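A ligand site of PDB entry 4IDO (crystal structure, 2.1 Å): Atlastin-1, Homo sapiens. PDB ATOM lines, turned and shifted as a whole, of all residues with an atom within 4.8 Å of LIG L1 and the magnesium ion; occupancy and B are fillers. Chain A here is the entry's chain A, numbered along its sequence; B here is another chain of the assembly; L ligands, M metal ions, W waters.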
ATOM      1  N   ALA A  75     -30.473  12.677 -21.862  1.00  0.00           N
ATOM      2  CA  ALA A  75     -29.792  11.516 -22.418  1.00  0.00           C
ATOM      3  C   ALA A  75     -30.126  10.259 -21.654  1.00  0.00           C
ATOM      4  O   ALA A  75     -30.330  10.294 -20.440  1.00  0.00           O
ATOM      5  CB  ALA A  75     -28.269  11.726 -22.447  1.00  0.00           C
ATOM      6  N   PHE A  76     -30.173   9.139 -22.376  1.00  0.00           N
ATOM      7  CA  PHE A  76     -30.553   7.884 -21.781  1.00  0.00           C
ATOM      8  C   PHE A  76     -29.455   7.314 -20.832  1.00  0.00           C
ATOM      9  O   PHE A  76     -28.281   7.723 -20.908  1.00  0.00           O
ATOM     10  CB  PHE A  76     -31.024   6.892 -22.885  1.00  0.00           C
ATOM     11  CG  PHE A  76     -29.913   6.061 -23.500  1.00  0.00           C
ATOM     12  CD1 PHE A  76     -28.914   6.629 -24.282  1.00  0.00           C
ATOM     13  CD2 PHE A  76     -29.901   4.680 -23.326  1.00  0.00           C
ATOM     14  CE1 PHE A  76     -27.909   5.843 -24.860  1.00  0.00           C
ATOM     15  CE2 PHE A  76     -28.885   3.894 -23.882  1.00  0.00           C
ATOM     16  CZ  PHE A  76     -27.892   4.472 -24.652  1.00  0.00           C
ATOM     17  N   ARG A  77     -29.865   6.445 -19.899  1.00  0.00           N
ATOM     18  CA  ARG A  77     -29.003   5.784 -18.918  1.00  0.00           C
ATOM     19  C   ARG A  77     -28.262   6.743 -17.941  1.00  0.00           C
ATOM     20  O   ARG A  77     -27.127   6.464 -17.536  1.00  0.00           O
ATOM     21  CB  ARG A  77     -27.954   4.885 -19.579  1.00  0.00           C
ATOM     22  CG  ARG A  77     -28.445   3.833 -20.549  1.00  0.00           C
ATOM     23  CD  ARG A  77     -29.091   2.619 -19.965  1.00  0.00           C
ATOM     24  NE  ARG A  77     -30.328   2.933 -19.261  1.00  0.00           N
ATOM     25  CZ  ARG A  77     -30.638   2.442 -18.065  1.00  0.00           C
ATOM     26  NH1 ARG A  77     -29.795   1.600 -17.466  1.00  0.00           N
ATOM     27  NH2 ARG A  77     -31.774   2.780 -17.470  1.00  0.00           N
ATOM     28  N   LYS A  78     -28.907   7.840 -17.552  1.00  0.00           N
ATOM     29  CA  LYS A  78     -28.261   8.838 -16.702  1.00  0.00           C
ATOM     30  C   LYS A  78     -28.981   9.065 -15.368  1.00  0.00           C
ATOM     31  O   LYS A  78     -28.733  10.077 -14.710  1.00  0.00           O
ATOM     32  CB  LYS A  78     -28.121  10.165 -17.423  1.00  0.00           C
ATOM     33  CG  LYS A  78     -27.358  10.151 -18.743  1.00  0.00           C
ATOM     34  CD  LYS A  78     -25.916   9.694 -18.606  1.00  0.00           C
ATOM     35  CE  LYS A  78     -25.146  10.089 -19.881  1.00  0.00           C
ATOM     36  NZ  LYS A  78     -23.762   9.542 -19.837  1.00  0.00           N
ATOM     37  N   GLY A  79     -29.852   8.148 -14.963  1.00  0.00           N
ATOM     38  CA  GLY A  79     -30.482   8.220 -13.651  1.00  0.00           C
ATOM     39  C   GLY A  79     -31.722   9.090 -13.482  1.00  0.00           C
ATOM     40  O   GLY A  79     -32.062   9.495 -12.366  1.00  0.00           O
ATOM     41  N   LYS A  80     -32.421   9.321 -14.591  1.00  0.00           N
ATOM     42  CA  LYS A  80     -33.644  10.133 -14.562  1.00  0.00           C
ATOM     43  C   LYS A  80     -34.759   9.464 -13.734  1.00  0.00           C
ATOM     44  O   LYS A  80     -35.372  10.091 -12.862  1.00  0.00           O
ATOM     45  CB  LYS A  80     -34.137  10.402 -15.996  1.00  0.00           C
ATOM     46  CG  LYS A  80     -33.184  11.214 -16.889  1.00  0.00           C
ATOM     47  CD  LYS A  80     -33.885  11.631 -18.225  1.00  0.00           C
ATOM     48  CE  LYS A  80     -34.198  10.388 -19.068  1.00  0.00           C
ATOM     49  NZ  LYS A  80     -33.003   9.459 -19.240  1.00  0.00           N
ATOM     50  N   SER A  81     -35.017   8.186 -13.990  1.00  0.00           N
ATOM     51  CA  SER A  81     -36.029   7.435 -13.243  1.00  0.00           C
ATOM     52  C   SER A  81     -35.738   7.289 -11.726  1.00  0.00           C
ATOM     53  O   SER A  81     -36.630   7.421 -10.892  1.00  0.00           O
ATOM     54  CB  SER A  81     -36.220   6.077 -13.884  1.00  0.00           C
ATOM     55  OG  SER A  81     -36.837   6.219 -15.144  1.00  0.00           O
ATOM     56  N   PHE A  82     -34.479   7.032 -11.400  1.00  0.00           N
ATOM     57  CA  PHE A  82     -33.942   7.043 -10.045  1.00  0.00           C
ATOM     58  C   PHE A  82     -34.302   8.353  -9.328  1.00  0.00           C
ATOM     59  O   PHE A  82     -34.810   8.361  -8.192  1.00  0.00           O
ATOM     60  CB  PHE A  82     -32.421   6.892 -10.201  1.00  0.00           C
ATOM     61  CG  PHE A  82     -31.632   6.831  -8.921  1.00  0.00           C
ATOM     62  CD1 PHE A  82     -31.365   5.599  -8.321  1.00  0.00           C
ATOM     63  CD2 PHE A  82     -31.070   7.972  -8.380  1.00  0.00           C
ATOM     64  CE1 PHE A  82     -30.606   5.524  -7.163  1.00  0.00           C
ATOM     65  CE2 PHE A  82     -30.288   7.900  -7.229  1.00  0.00           C
ATOM     66  CZ  PHE A  82     -30.067   6.673  -6.624  1.00  0.00           C
ATOM     67  N   SER A 111     -39.698   2.423 -13.014  1.00  0.00           N
ATOM     68  CA  SER A 111     -38.672   1.423 -13.119  1.00  0.00           C
ATOM     69  C   SER A 111     -37.306   2.020 -13.481  1.00  0.00           C
ATOM     70  O   SER A 111     -37.151   2.723 -14.476  1.00  0.00           O
ATOM     71  CB  SER A 111     -39.069   0.357 -14.126  1.00  0.00           C
ATOM     72  OG  SER A 111     -37.965  -0.492 -14.369  1.00  0.00           O
ATOM     73  N   TRP A 112     -36.300   1.703 -12.675  1.00  0.00           N
ATOM     74  CA  TRP A 112     -34.955   2.203 -12.902  1.00  0.00           C
ATOM     75  C   TRP A 112     -34.005   1.041 -12.702  1.00  0.00           C
ATOM     76  O   TRP A 112     -34.327   0.118 -11.957  1.00  0.00           O
ATOM     77  CB  TRP A 112     -34.633   3.335 -11.919  1.00  0.00           C
ATOM     78  CG  TRP A 112     -34.500   2.834 -10.494  1.00  0.00           C
ATOM     79  CD1 TRP A 112     -35.494   2.693  -9.584  1.00  0.00           C
ATOM     80  CD2 TRP A 112     -33.307   2.376  -9.853  1.00  0.00           C
ATOM     81  NE1 TRP A 112     -35.006   2.194  -8.406  1.00  0.00           N
ATOM     82  CE2 TRP A 112     -33.657   1.996  -8.544  1.00  0.00           C
ATOM     83  CE3 TRP A 112     -31.957   2.282 -10.245  1.00  0.00           C
ATOM     84  CZ2 TRP A 112     -32.721   1.500  -7.631  1.00  0.00           C
ATOM     85  CZ3 TRP A 112     -31.043   1.791  -9.348  1.00  0.00           C
ATOM     86  CH2 TRP A 112     -31.417   1.406  -8.046  1.00  0.00           C
ATOM     87  N   ARG A 113     -32.845   1.074 -13.359  1.00  0.00           N
ATOM     88  CA  ARG A 113     -31.832   0.011 -13.206  1.00  0.00           C
ATOM     89  C   ARG A 113     -30.552   0.346 -13.979  1.00  0.00           C
ATOM     90  O   ARG A 113     -30.543   1.222 -14.856  1.00  0.00           O
ATOM     91  CB  ARG A 113     -32.362  -1.333 -13.740  1.00  0.00           C
ATOM     92  CG  ARG A 113     -32.810  -1.277 -15.201  1.00  0.00           C
ATOM     93  CD  ARG A 113     -32.658  -2.646 -15.891  1.00  0.00           C
ATOM     94  NE  ARG A 113     -33.219  -2.609 -17.236  1.00  0.00           N
ATOM     95  CZ  ARG A 113     -32.594  -2.161 -18.318  1.00  0.00           C
ATOM     96  NH1 ARG A 113     -31.340  -1.692 -18.231  1.00  0.00           N
ATOM     97  NH2 ARG A 113     -33.206  -2.159 -19.492  1.00  0.00           N
ATOM     98  N   GLY A 114     -29.464  -0.371 -13.672  1.00  0.00           N
ATOM     99  CA  GLY A 114     -28.243  -0.232 -14.442  1.00  0.00           C
ATOM    100  C   GLY A 114     -28.307  -1.117 -15.676  1.00  0.00           C
ATOM    101  O   GLY A 114     -29.366  -1.644 -16.026  1.00  0.00           O
ATOM    102  N   THR A 120     -36.725   2.942 -19.580  1.00  0.00           N
ATOM    103  CA  THR A 120     -37.931   3.722 -19.840  1.00  0.00           C
ATOM    104  C   THR A 120     -38.109   3.959 -21.328  1.00  0.00           C
ATOM    105  O   THR A 120     -37.144   4.298 -22.005  1.00  0.00           O
ATOM    106  CB  THR A 120     -37.888   5.090 -19.127  1.00  0.00           C
ATOM    107  OG1 THR A 120     -37.493   4.921 -17.761  1.00  0.00           O
ATOM    108  CG2 THR A 120     -39.256   5.774 -19.178  1.00  0.00           C
ATOM    109  N   ASP A 146     -42.119  10.744 -16.264  1.00  0.00           N
ATOM    110  CA  ASP A 146     -40.811  10.136 -16.499  1.00  0.00           C
ATOM    111  C   ASP A 146     -40.667   9.846 -18.009  1.00  0.00           C
ATOM    112  O   ASP A 146     -41.608   9.389 -18.650  1.00  0.00           O
ATOM    113  CB  ASP A 146     -40.656   8.867 -15.657  1.00  0.00           C
ATOM    114  CG  ASP A 146     -39.222   8.358 -15.611  1.00  0.00           C
ATOM    115  OD1 ASP A 146     -38.279   9.144 -15.884  1.00  0.00           O
ATOM    116  OD2 ASP A 146     -39.050   7.155 -15.287  1.00  0.00           O
ATOM    117  N   THR A 147     -39.496  10.108 -18.590  1.00  0.00           N
ATOM    118  CA  THR A 147     -39.369  10.032 -20.051  1.00  0.00           C
ATOM    119  C   THR A 147     -38.267   9.099 -20.537  1.00  0.00           C
ATOM    120  O   THR A 147     -37.258   8.855 -19.862  1.00  0.00           O
ATOM    121  CB  THR A 147     -39.147  11.440 -20.692  1.00  0.00           C
ATOM    122  OG1 THR A 147     -37.819  11.932 -20.418  1.00  0.00           O
ATOM    123  CG2 THR A 147     -40.181  12.407 -20.167  1.00  0.00           C
ATOM    124  N   ARG A 217     -25.676  16.043 -13.224  1.00  0.00           N
ATOM    125  CA  ARG A 217     -25.272  14.878 -12.452  1.00  0.00           C
ATOM    126  C   ARG A 217     -23.756  14.722 -12.455  1.00  0.00           C
ATOM    127  O   ARG A 217     -23.083  15.122 -13.409  1.00  0.00           O
ATOM    128  CB  ARG A 217     -25.912  13.596 -13.025  1.00  0.00           C
ATOM    129  CG  ARG A 217     -27.426  13.672 -13.207  1.00  0.00           C
ATOM    130  CD  ARG A 217     -28.140  13.816 -11.869  1.00  0.00           C
ATOM    131  NE  ARG A 217     -28.444  12.516 -11.269  1.00  0.00           N
ATOM    132  CZ  ARG A 217     -29.607  11.890 -11.392  1.00  0.00           C
ATOM    133  NH1 ARG A 217     -30.574  12.434 -12.114  1.00  0.00           N
ATOM    134  NH2 ARG A 217     -29.786  10.704 -10.811  1.00  0.00           N
ATOM    135  N   ASP A 218     -23.228  14.140 -11.380  1.00  0.00           N
ATOM    136  CA  ASP A 218     -21.793  13.858 -11.281  1.00  0.00           C
ATOM    137  C   ASP A 218     -20.901  15.092 -11.491  1.00  0.00           C
ATOM    138  O   ASP A 218     -19.817  14.991 -12.043  1.00  0.00           O
ATOM    139  CB  ASP A 218     -21.382  12.750 -12.270  1.00  0.00           C
ATOM    140  CG  ASP A 218     -22.163  11.446 -12.063  1.00  0.00           C
ATOM    141  OD1 ASP A 218     -22.906  11.319 -11.082  1.00  0.00           O
ATOM    142  OD2 ASP A 218     -21.975  10.522 -12.860  1.00  0.00           O
ATOM    143  N   PRO A 270     -23.399  16.157  -6.785  1.00  0.00           N
ATOM    144  CA  PRO A 270     -22.243  15.267  -6.670  1.00  0.00           C
ATOM    145  C   PRO A 270     -22.552  13.881  -7.216  1.00  0.00           C
ATOM    146  O   PRO A 270     -23.725  13.495  -7.368  1.00  0.00           O
ATOM    147  CB  PRO A 270     -22.005  15.170  -5.152  1.00  0.00           C
ATOM    148  CG  PRO A 270     -22.733  16.307  -4.550  1.00  0.00           C
ATOM    149  CD  PRO A 270     -23.925  16.549  -5.463  1.00  0.00           C
ATOM    150  N   HIS A 271     -21.494  13.153  -7.558  1.00  0.00           N
ATOM    151  CA  HIS A 271     -21.595  11.749  -7.919  1.00  0.00           C
ATOM    152  C   HIS A 271     -22.122  11.018  -6.687  1.00  0.00           C
ATOM    153  O   HIS A 271     -21.721  11.340  -5.568  1.00  0.00           O
ATOM    154  CB  HIS A 271     -20.198  11.248  -8.310  1.00  0.00           C
ATOM    155  CG  HIS A 271     -20.208   9.929  -9.032  1.00  0.00           C
ATOM    156  ND1 HIS A 271     -20.537   8.741  -8.413  1.00  0.00           N
ATOM    157  CD2 HIS A 271     -19.880   9.613 -10.313  1.00  0.00           C
ATOM    158  CE1 HIS A 271     -20.438   7.758  -9.288  1.00  0.00           C
ATOM    159  NE2 HIS A 271     -20.054   8.261 -10.448  1.00  0.00           N
ATOM    160  N   PRO A 272     -23.057  10.050  -6.882  1.00  0.00           N
ATOM    161  CA  PRO A 272     -23.672   9.288  -5.770  1.00  0.00           C
ATOM    162  C   PRO A 272     -22.758   8.179  -5.235  1.00  0.00           C
ATOM    163  O   PRO A 272     -23.087   7.537  -4.239  1.00  0.00           O
ATOM    164  CB  PRO A 272     -24.921   8.676  -6.420  1.00  0.00           C
ATOM    165  CG  PRO A 272     -24.551   8.532  -7.858  1.00  0.00           C
ATOM    166  CD  PRO A 272     -23.730   9.766  -8.164  1.00  0.00           C
ATOM    167  N   VAL A 276     -23.335   2.914  -6.600  1.00  0.00           N
ATOM    168  CA  VAL A 276     -24.595   3.259  -7.240  1.00  0.00           C
ATOM    169  C   VAL A 276     -24.459   3.041  -8.744  1.00  0.00           C
ATOM    170  O   VAL A 276     -25.369   2.563  -9.409  1.00  0.00           O
ATOM    171  CB  VAL A 276     -25.007   4.736  -6.943  1.00  0.00           C
ATOM    172  CG1 VAL A 276     -26.197   5.139  -7.825  1.00  0.00           C
ATOM    173  CG2 VAL A 276     -25.350   4.899  -5.451  1.00  0.00           C
ATOM    174  N   ALA A 277     -23.297   3.384  -9.277  1.00  0.00           N
ATOM    175  CA  ALA A 277     -23.089   3.283 -10.723  1.00  0.00           C
ATOM    176  C   ALA A 277     -22.747   1.864 -11.201  1.00  0.00           C
ATOM    177  O   ALA A 277     -23.223   1.424 -12.262  1.00  0.00           O
ATOM    178  CB  ALA A 277     -22.040   4.296 -11.177  1.00  0.00           C
ATOM    179  N   PHE A 282     -27.055  -3.221  -6.354  1.00  0.00           N
ATOM    180  CA  PHE A 282     -27.519  -1.979  -5.757  1.00  0.00           C
ATOM    181  C   PHE A 282     -29.003  -1.803  -6.039  1.00  0.00           C
ATOM    182  O   PHE A 282     -29.424  -1.883  -7.195  1.00  0.00           O
ATOM    183  CB  PHE A 282     -26.740  -0.788  -6.324  1.00  0.00           C
ATOM    184  CG  PHE A 282     -27.270   0.537  -5.869  1.00  0.00           C
ATOM    185  CD1 PHE A 282     -27.213   0.899  -4.519  1.00  0.00           C
ATOM    186  CD2 PHE A 282     -27.850   1.426  -6.771  1.00  0.00           C
ATOM    187  CE1 PHE A 282     -27.706   2.120  -4.085  1.00  0.00           C
ATOM    188  CE2 PHE A 282     -28.348   2.652  -6.353  1.00  0.00           C
ATOM    189  CZ  PHE A 282     -28.268   3.007  -5.000  1.00  0.00           C
ATOM    190  N   PHE A 293     -23.885  13.296  -1.621  1.00  0.00           N
ATOM    191  CA  PHE A 293     -24.965  13.224  -2.609  1.00  0.00           C
ATOM    192  C   PHE A 293     -26.309  13.381  -1.913  1.00  0.00           C
ATOM    193  O   PHE A 293     -27.163  14.167  -2.341  1.00  0.00           O
ATOM    194  CB  PHE A 293     -24.921  11.886  -3.361  1.00  0.00           C
ATOM    195  CG  PHE A 293     -26.052  11.704  -4.335  1.00  0.00           C
ATOM    196  CD1 PHE A 293     -27.270  11.153  -3.919  1.00  0.00           C
ATOM    197  CD2 PHE A 293     -25.914  12.085  -5.667  1.00  0.00           C
ATOM    198  CE1 PHE A 293     -28.322  10.970  -4.818  1.00  0.00           C
ATOM    199  CE2 PHE A 293     -26.977  11.902  -6.588  1.00  0.00           C
ATOM    200  CZ  PHE A 293     -28.172  11.346  -6.156  1.00  0.00           C
ATOM    201  N   GLN B 180     -18.631   7.217 -20.513  1.00  0.00           N
ATOM    202  CA  GLN B 180     -19.662   6.299 -19.985  1.00  0.00           C
ATOM    203  C   GLN B 180     -20.292   5.318 -20.975  1.00  0.00           C
ATOM    204  O   GLN B 180     -20.578   4.158 -20.642  1.00  0.00           O
ATOM    205  CB  GLN B 180     -20.787   7.060 -19.247  1.00  0.00           C
ATOM    206  CG  GLN B 180     -20.369   7.796 -17.983  1.00  0.00           C
ATOM    207  CD  GLN B 180     -21.550   8.448 -17.261  1.00  0.00           C
ATOM    208  OE1 GLN B 180     -22.694   8.379 -17.716  1.00  0.00           O
ATOM    209  NE2 GLN B 180     -21.288   9.076 -16.131  1.00  0.00           N
HETATM  210  P1  LIG L   1     -32.510   6.593 -16.836  1.00  0.00           P
HETATM  211  O1  LIG L   1     -33.960   6.646 -16.353  1.00  0.00           O
HETATM  212  O2  LIG L   1     -31.947   7.965 -17.087  1.00  0.00           O
HETATM  213  O3  LIG L   1     -32.383   5.749 -18.064  1.00  0.00           O
HETATM  214  O4  LIG L   1     -31.536   5.914 -15.746  1.00  0.00           O
HETATM  215  P2  LIG L   1     -32.029   5.112 -14.433  1.00  0.00           P
HETATM  216  O5  LIG L   1     -32.805   6.044 -13.530  1.00  0.00           O
HETATM  217  O6  LIG L   1     -32.846   3.882 -14.770  1.00  0.00           O
HETATM  218  O7  LIG L   1     -30.608   4.754 -13.761  1.00  0.00           O
HETATM  219  C1  LIG L   1     -29.504   4.356 -14.561  1.00  0.00           C
HETATM  220  C2  LIG L   1     -28.298   4.028 -13.680  1.00  0.00           C
HETATM  221  O8  LIG L   1     -27.771   5.259 -13.187  1.00  0.00           O
HETATM  222  C3  LIG L   1     -28.604   3.209 -12.436  1.00  0.00           C
HETATM  223  O9  LIG L   1     -27.609   2.180 -12.299  1.00  0.00           O
HETATM  224  C4  LIG L   1     -28.442   4.167 -11.257  1.00  0.00           C
HETATM  225  O10 LIG L   1     -27.928   3.519 -10.097  1.00  0.00           O
HETATM  226  C5  LIG L   1     -27.394   5.093 -11.808  1.00  0.00           C
HETATM  227  N1  LIG L   1     -27.448   6.440 -11.246  1.00  0.00           N
HETATM  228  C6  LIG L   1     -28.502   7.063 -10.672  1.00  0.00           C
HETATM  229  N2  LIG L   1     -28.141   8.328 -10.367  1.00  0.00           N
HETATM  230  C7  LIG L   1     -26.865   8.519 -10.770  1.00  0.00           C
HETATM  231  C8  LIG L   1     -25.886   9.616 -10.760  1.00  0.00           C
HETATM  232  O11 LIG L   1     -26.216  10.715 -10.279  1.00  0.00           O
HETATM  233  N3  LIG L   1     -24.656   9.401 -11.289  1.00  0.00           N
HETATM  234  C9  LIG L   1     -24.305   8.217 -11.823  1.00  0.00           C
HETATM  235  N4  LIG L   1     -23.076   8.066 -12.345  1.00  0.00           N
HETATM  236  N5  LIG L   1     -25.157   7.153 -11.879  1.00  0.00           N
HETATM  237  C10 LIG L   1     -26.424   7.271 -11.374  1.00  0.00           C
HETATM  238 AL1  LG2 L   2     -33.580   5.417 -19.725  1.00  0.00          AL
HETATM  239  F1  LG2 L   2     -33.840   3.740 -19.196  1.00  0.00           F
HETATM  240  F2  LG2 L   2     -33.290   7.100 -20.268  1.00  0.00           F
HETATM  241  F3  LG2 L   2     -35.001   5.967 -18.846  1.00  0.00           F
HETATM  242  F4  LG2 L   2     -32.119   4.853 -20.578  1.00  0.00           F
HETATM  243 MG    MG M   1     -35.661   5.987 -16.967  1.00  0.00          MG
HETATM  244  O   HOH W   1     -25.850   9.797 -14.216  1.00  0.00           O
HETATM  245  O   HOH W   2     -25.202  13.266  -9.639  1.00  0.00           O
HETATM  246  O   HOH W   3     -26.186   7.299 -15.094  1.00  0.00           O
HETATM  247  O   HOH W   4     -36.409   7.911 -17.362  1.00  0.00           O
HETATM  248  O   HOH W   5     -25.419   2.898 -13.500  1.00  0.00           O
HETATM  249  O   HOH W   6     -35.126   4.167 -16.320  1.00  0.00           O
HETATM  250  O   HOH W   7     -21.987   5.867 -14.330  1.00  0.00           O
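Asp 146 touches the magnesium ion (OD2 to MG, 3.96 Å). Along chain A the residues within 4 Å of the magnesium ion span positions 81 to 146. The nearest printed residue that does not touch the magnesium ion is Ser 111 (4.4 Å).
The backbone carbonyl oxygen of Arg 113 is in hydrogen-bond range of the guanidinium group of Arg 77 (2.7 Å). The side-chain amino group of Lys 80 lies within hydrogen-bond range of the backbone carbonyl oxygen of Ala 75. The side-chain carboxylate (OD2) of Asp 146 sits close to the side-chain hydroxyl (OG) of Ser 81, at 2.4 Å. The backbone carbonyl oxygen (O) of Gly 79 sits at hydrogen-bond distance from the guanidinium group (NH2) of Arg 217, 3.0 Å away. The side-chain amide oxygen of Gln 180 of chain B lies within hydrogen-bond range of the side-chain amino group of Lys 78.
A nitrogen (N3) of LIG L1 sits at hydrogen-bond distance from the side-chain carboxylate (OD1) of Asp 218 (2.6 Å). The backbone NH (N) of Ser 81 sits at hydrogen-bond distance from an oxygen (O5) of LIG L1 (3.1 Å). O4 of LIG L1 sits at hydrogen-bond distance from N of Gly 79, at 2.9 Å. N of Thr 120 sits at hydrogen-bond distance from F1 of LG2 L2 (3.0 Å). NH2 of Arg 217 lies within hydrogen-bond range of N2 of LIG L1 (2.9 Å). An oxygen (O3) of LIG L1 sits close to the backbone NH (N) of Arg 77, at 3.2 Å. The guanidinium group (NH2) of Arg 77 lies within salt-bridge range of an oxygen (O6) of LIG L1, at 3.1 Å. N of Lys 78 lies within hydrogen-bond range of O2 of LIG L1 (3.1 Å). The backbone NH of Arg 77 sits at hydrogen-bond distance from a fluorine (F4) of LG2 L2 (2.8 Å). The backbone carbonyl oxygen (O) of Val 276 lies within hydrogen-bond range of an oxygen (O10) of LIG L1 (2.8 Å). The backbone NH (N) of Arg 113 lies within hydrogen-bond range of an oxygen (O6) of LIG L1, at 3.1 Å. The backbone NH of Phe 82 is in hydrogen-bond range of an oxygen (O5) of LIG L1. N of Gly 114 sits close to O9 of LIG L1. F1 of LG2 L2 is in hydrogen-bond range of NH2 of Arg 77. The side-chain amino group (NZ) of Lys 80 lies within hydrogen-bond range of a fluorine (F2) of LG2 L2, 2.6 Å away. An oxygen (O2) of LIG L1 is in hydrogen-bond range of the backbone NH (N) of Lys 80. The side-chain amino group (NZ) of Lys 80 lies within salt-bridge range of an oxygen (O2) of LIG L1, 2.8 Å away.
O1 of LIG L1 binds the magnesium ion (1.9 Å). A fluorine (F3) of LG2 L2 is bound to the magnesium ion (2.0 Å). Water W6 binds the magnesium ion, at 2.0 Å. Water W4 is bound to the magnesium ion (2.1 Å). OG of Ser 81 is bound to the magnesium ion, 2.2 Å away. The side-chain hydroxyl (OG1) of Thr 120 binds the magnesium ion (2.3 Å).
CA of Trp 112 touches O6 of LIG L1 (3.3 Å). His 271 touches LIG L1. Pro 272 touches LIG L1. Phe 282 touches LIG L1. CE2 of Phe 293 touches O11 of LIG L1, 3.95 Å away. Hydrophobic or aromatic side chains within 4 Å of LIG L1: Phe 82, Trp 112, Pro 272, Val 276, Phe 282 and Phe 293.
An aluminium atom (AL1) of LG2 L2 is bound by an oxygen (O3) of LIG L1, 2.1 Å away.
Water W4 bridges OD1 of Asp 146 (2.7 Å) and O of Thr 147 (2.8 Å). Water W6 lies within hydrogen-bond range of O6 of LIG L1 (2.8 Å) and O of Ser 111 (3.1 Å). Water W5 bridges O9 of LIG L1 (2.6 Å) and O of Ala 277 (2.9 Å). Water W2 lies within hydrogen-bond range of the backbone carbonyl oxygen (O) of Pro 270 (2.7 Å), the backbone NH (N) of Asp 218 (2.8 Å) and an oxygen (O11) of LIG L1 (2.8 Å). Water W1 lies within hydrogen-bond range of O of Lys 78 (2.9 Å) and N3 of LIG L1 (3.2 Å). Water W3 bridges O of Arg 77 (2.7 Å) and O8 of LIG L1 (3.2 Å).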
